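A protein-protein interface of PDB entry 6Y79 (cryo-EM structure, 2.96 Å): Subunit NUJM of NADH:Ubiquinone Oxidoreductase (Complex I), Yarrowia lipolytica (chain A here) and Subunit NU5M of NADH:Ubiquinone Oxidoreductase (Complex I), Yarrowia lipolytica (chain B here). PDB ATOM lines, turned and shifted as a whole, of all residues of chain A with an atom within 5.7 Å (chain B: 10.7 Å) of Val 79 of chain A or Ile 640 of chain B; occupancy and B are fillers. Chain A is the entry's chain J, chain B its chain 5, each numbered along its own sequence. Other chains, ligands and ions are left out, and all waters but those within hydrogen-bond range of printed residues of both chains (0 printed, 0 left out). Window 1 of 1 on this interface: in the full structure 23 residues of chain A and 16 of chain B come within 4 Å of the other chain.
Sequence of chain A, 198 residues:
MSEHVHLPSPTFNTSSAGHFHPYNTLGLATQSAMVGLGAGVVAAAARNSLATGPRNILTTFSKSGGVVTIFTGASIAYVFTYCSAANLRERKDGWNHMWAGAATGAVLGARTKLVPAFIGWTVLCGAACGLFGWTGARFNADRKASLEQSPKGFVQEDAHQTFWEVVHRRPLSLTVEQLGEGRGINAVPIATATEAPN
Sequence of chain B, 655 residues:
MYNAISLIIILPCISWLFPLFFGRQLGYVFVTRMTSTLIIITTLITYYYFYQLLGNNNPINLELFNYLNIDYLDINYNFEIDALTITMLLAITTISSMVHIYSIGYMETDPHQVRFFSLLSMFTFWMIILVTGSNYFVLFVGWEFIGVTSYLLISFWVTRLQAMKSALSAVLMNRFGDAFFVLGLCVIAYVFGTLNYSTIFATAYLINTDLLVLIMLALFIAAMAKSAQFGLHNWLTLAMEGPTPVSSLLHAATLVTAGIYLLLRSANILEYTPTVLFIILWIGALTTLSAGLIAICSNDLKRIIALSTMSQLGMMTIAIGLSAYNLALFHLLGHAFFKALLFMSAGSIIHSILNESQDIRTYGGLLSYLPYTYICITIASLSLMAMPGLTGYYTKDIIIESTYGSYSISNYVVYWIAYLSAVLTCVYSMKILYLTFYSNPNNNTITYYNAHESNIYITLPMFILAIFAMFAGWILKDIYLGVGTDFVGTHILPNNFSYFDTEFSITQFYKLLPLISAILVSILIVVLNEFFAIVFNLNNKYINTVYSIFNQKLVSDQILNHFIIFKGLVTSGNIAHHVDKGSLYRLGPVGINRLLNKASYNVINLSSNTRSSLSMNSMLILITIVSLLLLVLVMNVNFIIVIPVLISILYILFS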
ATOM      1  N   THR A  25      10.593  -9.524  -3.770  1.00  0.00           N
ATOM      2  CA  THR A  25      11.190  -8.390  -3.061  1.00  0.00           C
ATOM      3  C   THR A  25      12.640  -8.182  -3.481  1.00  0.00           C
ATOM      4  O   THR A  25      13.098  -7.032  -3.631  1.00  0.00           O
ATOM      5  CB  THR A  25      11.096  -8.581  -1.552  1.00  0.00           C
ATOM      6  OG1 THR A  25       9.785  -9.011  -1.188  1.00  0.00           O
ATOM      7  CG2 THR A  25      11.379  -7.275  -0.834  1.00  0.00           C
ATOM      8  N   LEU A  28      12.452  -6.865  -7.544  1.00  0.00           N
ATOM      9  CA  LEU A  28      11.839  -5.543  -7.599  1.00  0.00           C
ATOM     10  C   LEU A  28      12.686  -4.524  -6.865  1.00  0.00           C
ATOM     11  O   LEU A  28      12.771  -3.379  -7.312  1.00  0.00           O
ATOM     12  CB  LEU A  28      10.429  -5.535  -7.013  1.00  0.00           C
ATOM     13  CG  LEU A  28       9.137  -5.804  -7.796  1.00  0.00           C
ATOM     14  CD1 LEU A  28       9.090  -4.832  -8.909  1.00  0.00           C
ATOM     15  CD2 LEU A  28       8.994  -7.235  -8.344  1.00  0.00           C
ATOM     16  N   ALA A  29      13.339  -4.913  -5.763  1.00  0.00           N
ATOM     17  CA  ALA A  29      14.243  -3.976  -5.108  1.00  0.00           C
ATOM     18  C   ALA A  29      15.504  -3.728  -5.938  1.00  0.00           C
ATOM     19  O   ALA A  29      16.010  -2.598  -5.960  1.00  0.00           O
ATOM     20  CB  ALA A  29      14.587  -4.477  -3.711  1.00  0.00           C
ATOM     21  N   SER A  32      14.352  -1.358  -8.684  1.00  0.00           N
ATOM     22  CA  SER A  32      14.171  -0.042  -8.088  1.00  0.00           C
ATOM     23  C   SER A  32      15.494   0.649  -7.825  1.00  0.00           C
ATOM     24  O   SER A  32      15.589   1.870  -7.969  1.00  0.00           O
ATOM     25  CB  SER A  32      13.410  -0.180  -6.777  1.00  0.00           C
ATOM     26  OG  SER A  32      12.194  -0.838  -6.987  1.00  0.00           O
ATOM     27  N   ALA A  74      15.152   6.375  -1.378  1.00  0.00           N
ATOM     28  CA  ALA A  74      13.698   6.329  -1.455  1.00  0.00           C
ATOM     29  C   ALA A  74      13.212   5.124  -2.256  1.00  0.00           C
ATOM     30  O   ALA A  74      12.240   4.470  -1.858  1.00  0.00           O
ATOM     31  CB  ALA A  74      13.167   7.626  -2.061  1.00  0.00           C
ATOM     32  N   SER A  75      13.893   4.796  -3.360  1.00  0.00           N
ATOM     33  CA  SER A  75      13.450   3.689  -4.208  1.00  0.00           C
ATOM     34  C   SER A  75      13.569   2.342  -3.502  1.00  0.00           C
ATOM     35  O   SER A  75      12.589   1.574  -3.447  1.00  0.00           O
ATOM     36  CB  SER A  75      14.242   3.695  -5.512  1.00  0.00           C
ATOM     37  OG  SER A  75      13.998   4.889  -6.239  1.00  0.00           O
ATOM     38  N   ILE A  76      14.758   2.052  -2.939  1.00  0.00           N
ATOM     39  CA  ILE A  76      14.973   0.825  -2.166  1.00  0.00           C
ATOM     40  C   ILE A  76      13.998   0.738  -0.998  1.00  0.00           C
ATOM     41  O   ILE A  76      13.344  -0.297  -0.814  1.00  0.00           O
ATOM     42  CB  ILE A  76      16.427   0.713  -1.662  1.00  0.00           C
ATOM     43  CG1 ILE A  76      17.481   0.851  -2.754  1.00  0.00           C
ATOM     44  CG2 ILE A  76      16.630  -0.623  -0.960  1.00  0.00           C
ATOM     45  CD1 ILE A  76      18.878   1.046  -2.157  1.00  0.00           C
ATOM     46  N   ALA A  77      13.839   1.833  -0.232  1.00  0.00           N
ATOM     47  CA  ALA A  77      13.011   1.800   0.973  1.00  0.00           C
ATOM     48  C   ALA A  77      11.544   1.554   0.658  1.00  0.00           C
ATOM     49  O   ALA A  77      10.919   0.672   1.265  1.00  0.00           O
ATOM     50  CB  ALA A  77      13.156   3.100   1.752  1.00  0.00           C
ATOM     51  N   TYR A  78      10.987   2.303  -0.305  1.00  0.00           N
ATOM     52  CA  TYR A  78       9.571   2.163  -0.624  1.00  0.00           C
ATOM     53  C   TYR A  78       9.268   0.786  -1.183  1.00  0.00           C
ATOM     54  O   TYR A  78       8.309   0.145  -0.753  1.00  0.00           O
ATOM     55  CB  TYR A  78       9.120   3.240  -1.613  1.00  0.00           C
ATOM     56  CG  TYR A  78       7.623   3.244  -1.931  1.00  0.00           C
ATOM     57  CD1 TYR A  78       7.093   2.465  -2.963  1.00  0.00           C
ATOM     58  CD2 TYR A  78       6.748   4.048  -1.215  1.00  0.00           C
ATOM     59  CE1 TYR A  78       5.748   2.457  -3.236  1.00  0.00           C
ATOM     60  CE2 TYR A  78       5.395   4.049  -1.491  1.00  0.00           C
ATOM     61  CZ  TYR A  78       4.904   3.254  -2.500  1.00  0.00           C
ATOM     62  OH  TYR A  78       3.560   3.265  -2.773  1.00  0.00           O
ATOM     63  N   VAL A  79      10.063   0.303  -2.139  1.00  0.00           N
ATOM     64  CA  VAL A  79       9.645  -0.946  -2.772  1.00  0.00           C
ATOM     65  C   VAL A  79       9.954  -2.156  -1.890  1.00  0.00           C
ATOM     66  O   VAL A  79       9.179  -3.126  -1.870  1.00  0.00           O
ATOM     67  CB  VAL A  79      10.265  -1.043  -4.170  1.00  0.00           C
ATOM     68  CG1 VAL A  79       9.683  -2.208  -4.919  1.00  0.00           C
ATOM     69  CG2 VAL A  79       9.939   0.221  -4.914  1.00  0.00           C
ATOM     70  N   PHE A  80      11.023  -2.090  -1.087  1.00  0.00           N
ATOM     71  CA  PHE A  80      11.287  -3.132  -0.101  1.00  0.00           C
ATOM     72  C   PHE A  80      10.179  -3.214   0.935  1.00  0.00           C
ATOM     73  O   PHE A  80       9.651  -4.303   1.185  1.00  0.00           O
ATOM     74  CB  PHE A  80      12.631  -2.881   0.588  1.00  0.00           C
ATOM     75  CG  PHE A  80      13.041  -3.971   1.536  1.00  0.00           C
ATOM     76  CD1 PHE A  80      13.584  -5.148   1.052  1.00  0.00           C
ATOM     77  CD2 PHE A  80      12.865  -3.830   2.906  1.00  0.00           C
ATOM     78  CE1 PHE A  80      13.946  -6.168   1.913  1.00  0.00           C
ATOM     79  CE2 PHE A  80      13.227  -4.850   3.774  1.00  0.00           C
ATOM     80  CZ  PHE A  80      13.769  -6.018   3.273  1.00  0.00           C
ATOM     81  N   THR A  81       9.787  -2.071   1.519  1.00  0.00           N
ATOM     82  CA  THR A  81       8.760  -2.083   2.552  1.00  0.00           C
ATOM     83  C   THR A  81       7.386  -2.411   1.982  1.00  0.00           C
ATOM     84  O   THR A  81       6.611  -3.114   2.640  1.00  0.00           O
ATOM     85  CB  THR A  81       8.755  -0.742   3.270  1.00  0.00           C
ATOM     86  OG1 THR A  81      10.090  -0.441   3.673  1.00  0.00           O
ATOM     87  CG2 THR A  81       7.872  -0.777   4.499  1.00  0.00           C
ATOM     88  N   TYR A  82       7.094  -1.974   0.750  1.00  0.00           N
ATOM     89  CA  TYR A  82       5.815  -2.285   0.119  1.00  0.00           C
ATOM     90  C   TYR A  82       5.665  -3.776  -0.126  1.00  0.00           C
ATOM     91  O   TYR A  82       4.663  -4.382   0.272  1.00  0.00           O
ATOM     92  CB  TYR A  82       5.674  -1.540  -1.208  1.00  0.00           C
ATOM     93  CG  TYR A  82       4.377  -1.857  -1.922  1.00  0.00           C
ATOM     94  CD1 TYR A  82       3.189  -1.277  -1.515  1.00  0.00           C
ATOM     95  CD2 TYR A  82       4.335  -2.750  -2.988  1.00  0.00           C
ATOM     96  CE1 TYR A  82       2.005  -1.569  -2.148  1.00  0.00           C
ATOM     97  CE2 TYR A  82       3.152  -3.051  -3.614  1.00  0.00           C
ATOM     98  CZ  TYR A  82       1.994  -2.457  -3.190  1.00  0.00           C
ATOM     99  OH  TYR A  82       0.810  -2.746  -3.818  1.00  0.00           O
ATOM    100  N   CYS A  83       6.644  -4.380  -0.810  1.00  0.00           N
ATOM    101  CA  CYS A  83       6.549  -5.800  -1.127  1.00  0.00           C
ATOM    102  C   CYS A  83       6.676  -6.666   0.111  1.00  0.00           C
ATOM    103  O   CYS A  83       6.005  -7.706   0.205  1.00  0.00           O
ATOM    104  CB  CYS A  83       7.592  -6.185  -2.170  1.00  0.00           C
ATOM    105  SG  CYS A  83       7.475  -5.244  -3.694  1.00  0.00           S
ATOM    106  N   SER A  84       7.470  -6.226   1.096  1.00  0.00           N
ATOM    107  CA  SER A  84       7.554  -6.988   2.329  1.00  0.00           C
ATOM    108  C   SER A  84       6.240  -6.934   3.105  1.00  0.00           C
ATOM    109  O   SER A  84       5.769  -7.956   3.581  1.00  0.00           O
ATOM    110  CB  SER A  84       8.701  -6.478   3.190  1.00  0.00           C
ATOM    111  OG  SER A  84       8.745  -7.193   4.410  1.00  0.00           O
ATOM    112  N   HIS A  97       0.857   0.690   1.058  1.00  0.00           N
ATOM    113  CA  HIS A  97       1.322   2.009   0.660  1.00  0.00           C
ATOM    114  C   HIS A  97       1.545   2.905   1.864  1.00  0.00           C
ATOM    115  O   HIS A  97       2.468   3.726   1.845  1.00  0.00           O
ATOM    116  CB  HIS A  97       0.336   2.641  -0.314  1.00  0.00           C
ATOM    117  CG  HIS A  97       0.257   1.930  -1.624  1.00  0.00           C
ATOM    118  ND1 HIS A  97       1.180   2.117  -2.627  1.00  0.00           N
ATOM    119  CD2 HIS A  97      -0.624   1.015  -2.087  1.00  0.00           C
ATOM    120  CE1 HIS A  97       0.865   1.356  -3.657  1.00  0.00           C
ATOM    121  NE2 HIS A  97      -0.224   0.675  -3.354  1.00  0.00           N
ATOM    122  N   ALA A 100       4.985   1.588   3.307  1.00  0.00           N
ATOM    123  CA  ALA A 100       6.075   1.947   2.410  1.00  0.00           C
ATOM    124  C   ALA A 100       6.317   3.450   2.370  1.00  0.00           C
ATOM    125  O   ALA A 100       7.471   3.887   2.272  1.00  0.00           O
ATOM    126  CB  ALA A 100       5.778   1.418   1.018  1.00  0.00           C
ATOM    127  N   LEU B 631      10.409   8.608 -17.455  1.00  0.00           N
ATOM    128  CA  LEU B 631       9.443   8.144 -16.467  1.00  0.00           C
ATOM    129  C   LEU B 631       8.482   7.127 -17.055  1.00  0.00           C
ATOM    130  O   LEU B 631       8.197   6.109 -16.424  1.00  0.00           O
ATOM    131  CB  LEU B 631       8.649   9.314 -15.899  1.00  0.00           C
ATOM    132  CG  LEU B 631       9.273  10.228 -14.855  1.00  0.00           C
ATOM    133  CD1 LEU B 631       8.367  11.418 -14.645  1.00  0.00           C
ATOM    134  CD2 LEU B 631       9.492   9.484 -13.566  1.00  0.00           C
ATOM    135  N   LEU B 633       9.041   5.297 -19.696  1.00  0.00           N
ATOM    136  CA  LEU B 633       9.879   4.128 -19.956  1.00  0.00           C
ATOM    137  C   LEU B 633       9.971   3.229 -18.730  1.00  0.00           C
ATOM    138  O   LEU B 633       9.905   2.000 -18.845  1.00  0.00           O
ATOM    139  CB  LEU B 633      11.269   4.581 -20.387  1.00  0.00           C
ATOM    140  CG  LEU B 633      12.336   3.510 -20.623  1.00  0.00           C
ATOM    141  CD1 LEU B 633      11.904   2.582 -21.736  1.00  0.00           C
ATOM    142  CD2 LEU B 633      13.673   4.153 -20.944  1.00  0.00           C
ATOM    143  N   VAL B 634      10.157   3.830 -17.549  1.00  0.00           N
ATOM    144  CA  VAL B 634      10.085   3.078 -16.293  1.00  0.00           C
ATOM    145  C   VAL B 634       8.681   2.529 -16.079  1.00  0.00           C
ATOM    146  O   VAL B 634       8.488   1.394 -15.632  1.00  0.00           O
ATOM    147  CB  VAL B 634      10.506   3.979 -15.116  1.00  0.00           C
ATOM    148  CG1 VAL B 634      10.317   3.287 -13.789  1.00  0.00           C
ATOM    149  CG2 VAL B 634      11.924   4.399 -15.252  1.00  0.00           C
ATOM    150  N   MET B 635       7.687   3.313 -16.446  1.00  0.00           N
ATOM    151  CA  MET B 635       6.359   3.209 -15.869  1.00  0.00           C
ATOM    152  C   MET B 635       5.503   2.167 -16.577  1.00  0.00           C
ATOM    153  O   MET B 635       4.584   1.610 -15.969  1.00  0.00           O
ATOM    154  CB  MET B 635       5.757   4.613 -15.902  1.00  0.00           C
ATOM    155  CG  MET B 635       4.305   4.832 -15.657  1.00  0.00           C
ATOM    156  SD  MET B 635       4.049   6.569 -16.098  1.00  0.00           S
ATOM    157  CE  MET B 635       5.179   7.401 -14.985  1.00  0.00           C
ATOM    158  N   ASN B 636       5.789   1.863 -17.847  1.00  0.00           N
ATOM    159  CA  ASN B 636       5.079   0.730 -18.438  1.00  0.00           C
ATOM    160  C   ASN B 636       5.720  -0.613 -18.095  1.00  0.00           C
ATOM    161  O   ASN B 636       5.061  -1.652 -18.230  1.00  0.00           O
ATOM    162  CB  ASN B 636       4.928   0.894 -19.957  1.00  0.00           C
ATOM    163  CG  ASN B 636       6.247   1.024 -20.695  1.00  0.00           C
ATOM    164  OD1 ASN B 636       7.332   0.915 -20.125  1.00  0.00           O
ATOM    165  ND2 ASN B 636       6.149   1.280 -21.990  1.00  0.00           N
ATOM    166  N   VAL B 637       6.983  -0.610 -17.667  1.00  0.00           N
ATOM    167  CA  VAL B 637       7.598  -1.822 -17.133  1.00  0.00           C
ATOM    168  C   VAL B 637       6.917  -2.228 -15.835  1.00  0.00           C
ATOM    169  O   VAL B 637       6.346  -3.317 -15.722  1.00  0.00           O
ATOM    170  CB  VAL B 637       9.105  -1.609 -16.917  1.00  0.00           C
ATOM    171  CG1 VAL B 637       9.734  -2.826 -16.255  1.00  0.00           C
ATOM    172  CG2 VAL B 637       9.788  -1.299 -18.228  1.00  0.00           C
ATOM    173  N   ASN B 638       6.958  -1.350 -14.844  1.00  0.00           N
ATOM    174  CA  ASN B 638       6.357  -1.613 -13.549  1.00  0.00           C
ATOM    175  C   ASN B 638       5.962  -0.293 -12.912  1.00  0.00           C
ATOM    176  O   ASN B 638       6.727   0.674 -12.955  1.00  0.00           O
ATOM    177  CB  ASN B 638       7.323  -2.363 -12.640  1.00  0.00           C
ATOM    178  CG  ASN B 638       6.663  -2.844 -11.387  1.00  0.00           C
ATOM    179  OD1 ASN B 638       5.613  -3.476 -11.423  1.00  0.00           O
ATOM    180  ND2 ASN B 638       7.238  -2.489 -10.264  1.00  0.00           N
ATOM    181  N   PHE B 639       4.768  -0.254 -12.323  1.00  0.00           N
ATOM    182  CA  PHE B 639       4.275   0.975 -11.722  1.00  0.00           C
ATOM    183  C   PHE B 639       4.746   1.150 -10.283  1.00  0.00           C
ATOM    184  O   PHE B 639       4.722   2.269  -9.765  1.00  0.00           O
ATOM    185  CB  PHE B 639       2.745   1.006 -11.809  1.00  0.00           C
ATOM    186  CG  PHE B 639       2.136   2.278 -11.303  1.00  0.00           C
ATOM    187  CD1 PHE B 639       2.217   3.447 -12.041  1.00  0.00           C
ATOM    188  CD2 PHE B 639       1.516   2.310 -10.068  1.00  0.00           C
ATOM    189  CE1 PHE B 639       1.675   4.620 -11.557  1.00  0.00           C
ATOM    190  CE2 PHE B 639       0.978   3.473  -9.582  1.00  0.00           C
ATOM    191  CZ  PHE B 639       1.053   4.630 -10.327  1.00  0.00           C
ATOM    192  N   ILE B 640       5.198   0.081  -9.629  1.00  0.00           N
ATOM    193  CA  ILE B 640       5.661   0.212  -8.253  1.00  0.00           C
ATOM    194  C   ILE B 640       6.997   0.946  -8.198  1.00  0.00           C
ATOM    195  O   ILE B 640       7.248   1.725  -7.273  1.00  0.00           O
ATOM    196  CB  ILE B 640       5.725  -1.182  -7.596  1.00  0.00           C
ATOM    197  CG1 ILE B 640       4.352  -1.841  -7.641  1.00  0.00           C
ATOM    198  CG2 ILE B 640       6.190  -1.111  -6.153  1.00  0.00           C
ATOM    199  CD1 ILE B 640       3.301  -1.072  -6.881  1.00  0.00           C
ATOM    200  N   ILE B 641       7.844   0.781  -9.213  1.00  0.00           N
ATOM    201  CA  ILE B 641       9.202   1.309  -9.153  1.00  0.00           C
ATOM    202  C   ILE B 641       9.256   2.769  -9.584  1.00  0.00           C
ATOM    203  O   ILE B 641      10.338   3.364  -9.636  1.00  0.00           O
ATOM    204  CB  ILE B 641      10.162   0.455 -10.001  1.00  0.00           C
ATOM    205  CG1 ILE B 641       9.775   0.488 -11.471  1.00  0.00           C
ATOM    206  CG2 ILE B 641      10.136  -0.978  -9.541  1.00  0.00           C
ATOM    207  CD1 ILE B 641      10.773  -0.222 -12.367  1.00  0.00           C
ATOM    208  N   VAL B 642       8.103   3.366  -9.880  1.00  0.00           N
ATOM    209  CA  VAL B 642       8.049   4.754 -10.317  1.00  0.00           C
ATOM    210  C   VAL B 642       7.377   5.664  -9.290  1.00  0.00           C
ATOM    211  O   VAL B 642       7.582   6.886  -9.343  1.00  0.00           O
ATOM    212  CB  VAL B 642       7.360   4.875 -11.698  1.00  0.00           C
ATOM    213  CG1 VAL B 642       5.858   4.766 -11.590  1.00  0.00           C
ATOM    214  CG2 VAL B 642       7.783   6.142 -12.450  1.00  0.00           C
ATOM    215  N   ILE B 643       6.605   5.109  -8.352  1.00  0.00           N
ATOM    216  CA  ILE B 643       6.124   5.883  -7.201  1.00  0.00           C
ATOM    217  C   ILE B 643       7.241   6.532  -6.369  1.00  0.00           C
ATOM    218  O   ILE B 643       7.136   7.733  -6.082  1.00  0.00           O
ATOM    219  CB  ILE B 643       5.170   5.027  -6.354  1.00  0.00           C
ATOM    220  CG1 ILE B 643       3.987   4.582  -7.202  1.00  0.00           C
ATOM    221  CG2 ILE B 643       4.685   5.786  -5.143  1.00  0.00           C
ATOM    222  CD1 ILE B 643       3.079   3.634  -6.501  1.00  0.00           C
ATOM    223  N   PRO B 644       8.321   5.830  -5.965  1.00  0.00           N
ATOM    224  CA  PRO B 644       9.350   6.543  -5.196  1.00  0.00           C
ATOM    225  C   PRO B 644      10.160   7.506  -6.032  1.00  0.00           C
ATOM    226  O   PRO B 644      10.711   8.459  -5.472  1.00  0.00           O
ATOM    227  CB  PRO B 644      10.239   5.424  -4.652  1.00  0.00           C
ATOM    228  CG  PRO B 644       9.588   4.191  -4.999  1.00  0.00           C
ATOM    229  CD  PRO B 644       8.746   4.427  -6.140  1.00  0.00           C
ATOM    230  N   VAL B 645      10.248   7.288  -7.348  1.00  0.00           N
ATOM    231  CA  VAL B 645      10.878   8.264  -8.232  1.00  0.00           C
ATOM    232  C   VAL B 645      10.119   9.580  -8.189  1.00  0.00           C
ATOM    233  O   VAL B 645      10.717  10.655  -8.082  1.00  0.00           O
ATOM    234  CB  VAL B 645      10.969   7.711  -9.666  1.00  0.00           C
ATOM    235  CG1 VAL B 645      11.646   8.709 -10.584  1.00  0.00           C
ATOM    236  CG2 VAL B 645      11.709   6.394  -9.680  1.00  0.00           C
ATOM    237  N   LEU B 646       8.787   9.514  -8.204  1.00  0.00           N
ATOM    238  CA  LEU B 646       7.983  10.730  -8.177  1.00  0.00           C
ATOM    239  C   LEU B 646       7.961  11.367  -6.798  1.00  0.00           C
ATOM    240  O   LEU B 646       7.931  12.599  -6.697  1.00  0.00           O
ATOM    241  CB  LEU B 646       6.572  10.417  -8.648  1.00  0.00           C
ATOM    242  CG  LEU B 646       6.624   9.951 -10.097  1.00  0.00           C
ATOM    243  CD1 LEU B 646       5.308   9.392 -10.530  1.00  0.00           C
ATOM    244  CD2 LEU B 646       7.054  11.075 -11.009  1.00  0.00           C
ATOM    245  N   ILE B 647       7.995  10.554  -5.738  1.00  0.00           N
ATOM    246  CA  ILE B 647       8.179  11.081  -4.386  1.00  0.00           C
ATOM    247  C   ILE B 647       9.521  11.799  -4.269  1.00  0.00           C
ATOM    248  O   ILE B 647       9.618  12.867  -3.650  1.00  0.00           O
ATOM    249  CB  ILE B 647       8.044   9.943  -3.356  1.00  0.00           C
ATOM    250  CG1 ILE B 647       6.598   9.465  -3.270  1.00  0.00           C
ATOM    251  CG2 ILE B 647       8.505  10.371  -1.976  1.00  0.00           C
ATOM    252  CD1 ILE B 647       6.460   8.143  -2.563  1.00  0.00           C
ATOM    253  N   SER B 648      10.563  11.264  -4.908  1.00  0.00           N
ATOM    254  CA  SER B 648      11.855  11.923  -4.807  1.00  0.00           C
ATOM    255  C   SER B 648      11.876  13.195  -5.648  1.00  0.00           C
ATOM    256  O   SER B 648      12.521  14.175  -5.273  1.00  0.00           O
ATOM    257  CB  SER B 648      12.962  10.957  -5.210  1.00  0.00           C
ATOM    258  OG  SER B 648      12.648   9.629  -4.803  1.00  0.00           O
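SG of Cys 83 of chain A sits at hydrogen-bond distance from O of Val 79 of chain A.
N of Ile 641 of chain B lies close to ND2 of Asn 638 of chain B (3.5 Å).
The side-chain hydroxyl (OH) of Tyr 78 of chain A sits at hydrogen-bond distance from a ring nitrogen (ND1) of His 97 of chain A, at 2.6 Å.
The backbone carbonyl oxygen (O) of Leu 28 of chain A sits at hydrogen-bond distance from the side-chain hydroxyl (OG) of Ser 32 of chain A, 2.6 Å away.
The side-chain amide nitrogen of Asn 638 of chain B lies close to the backbone NH of Ile 640 of chain B.
Among the printed residues, merely in contact across the chains: Leu 28 of chain A with Asn 638 of chain B, Ser 32 of chain A with Ile 641 of chain B, Ala 74 of chain A with Ser 648 of chain B, Tyr 78 of chain A with Pro 644 of chain B, Ala 74 of chain A with Pro 644 of chain B, Tyr 78 of chain A with Ile 643 of chain B, Ser 75 of chain A with Pro 644 of chain B, Tyr 82 of chain A with Ile 640 of chain B, Val 79 of chain A with Ile 640 of chain B and Val 79 of chain A with Pro 644 of chain B.
No residue of chain B comes within 4 Å of Ala 29 of chain A.
Ser 32 of chain A touches one residue of chain B.
Printed residues of chain B within 4 Å of Ala 74 of chain A: Pro 644 (3.6 Å) and Ser 648 (3.4 Å).
No residue of chain B comes within 4 Å of Ala 77 of chain A.
Tyr 78 of chain A touches two residues of chain B.
Of the printed residues of chain B, Val 79 of chain A touches Ile 640 (3.9 Å) and Pro 644 (3.99 Å).
Thr 81 of chain A touches none of the printed residues of chain B.
No residue of chain B comes within 4 Å of Cys 83 of chain A.
Of the printed residues of chain A, Asn 638 of chain B touches Leu 28 (3.3 Å).
Ile 640 of chain B touches just these residues of chain A: Val 79 (3.9 Å) and Tyr 82 (3.8 Å).
Of the printed residues of chain A, Ile 641 of chain B touches Ser 32.
Val 642 of chain B touches none of the printed residues of chain A.
Of the printed residues of chain A, Ile 643 of chain B touches Tyr 78 (3.6 Å).
Of the printed residues of chain A, Pro 644 of chain B touches Ala 74 (3.6 Å), Ser 75 (3.7 Å), Tyr 78 (3.5 Å) and Val 79 (3.99 Å).
The nearest printed residue of chain B that does not touch Val 79 of chain A is Ile 641 of chain B (4.4 Å).
The nearest residue of chain A that does not touch Ile 640 of chain B is Tyr 78 of chain A (4.4 Å).
Hydrophobic or aromatic side chains of chain A that line the printed part of chain B: Leu 28, Ala 74, Tyr 78, Val 79 and Tyr 82.
Of the 17 printed residues of chain B, 6 touch a printed residue of chain A.
Hydrophobic or aromatic side chains of chain B that line the printed part of chain A: Ile 640, Ile 641, Ile 643 and Pro 644.
Among the printed residues, 10 pairs touch across the chains.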
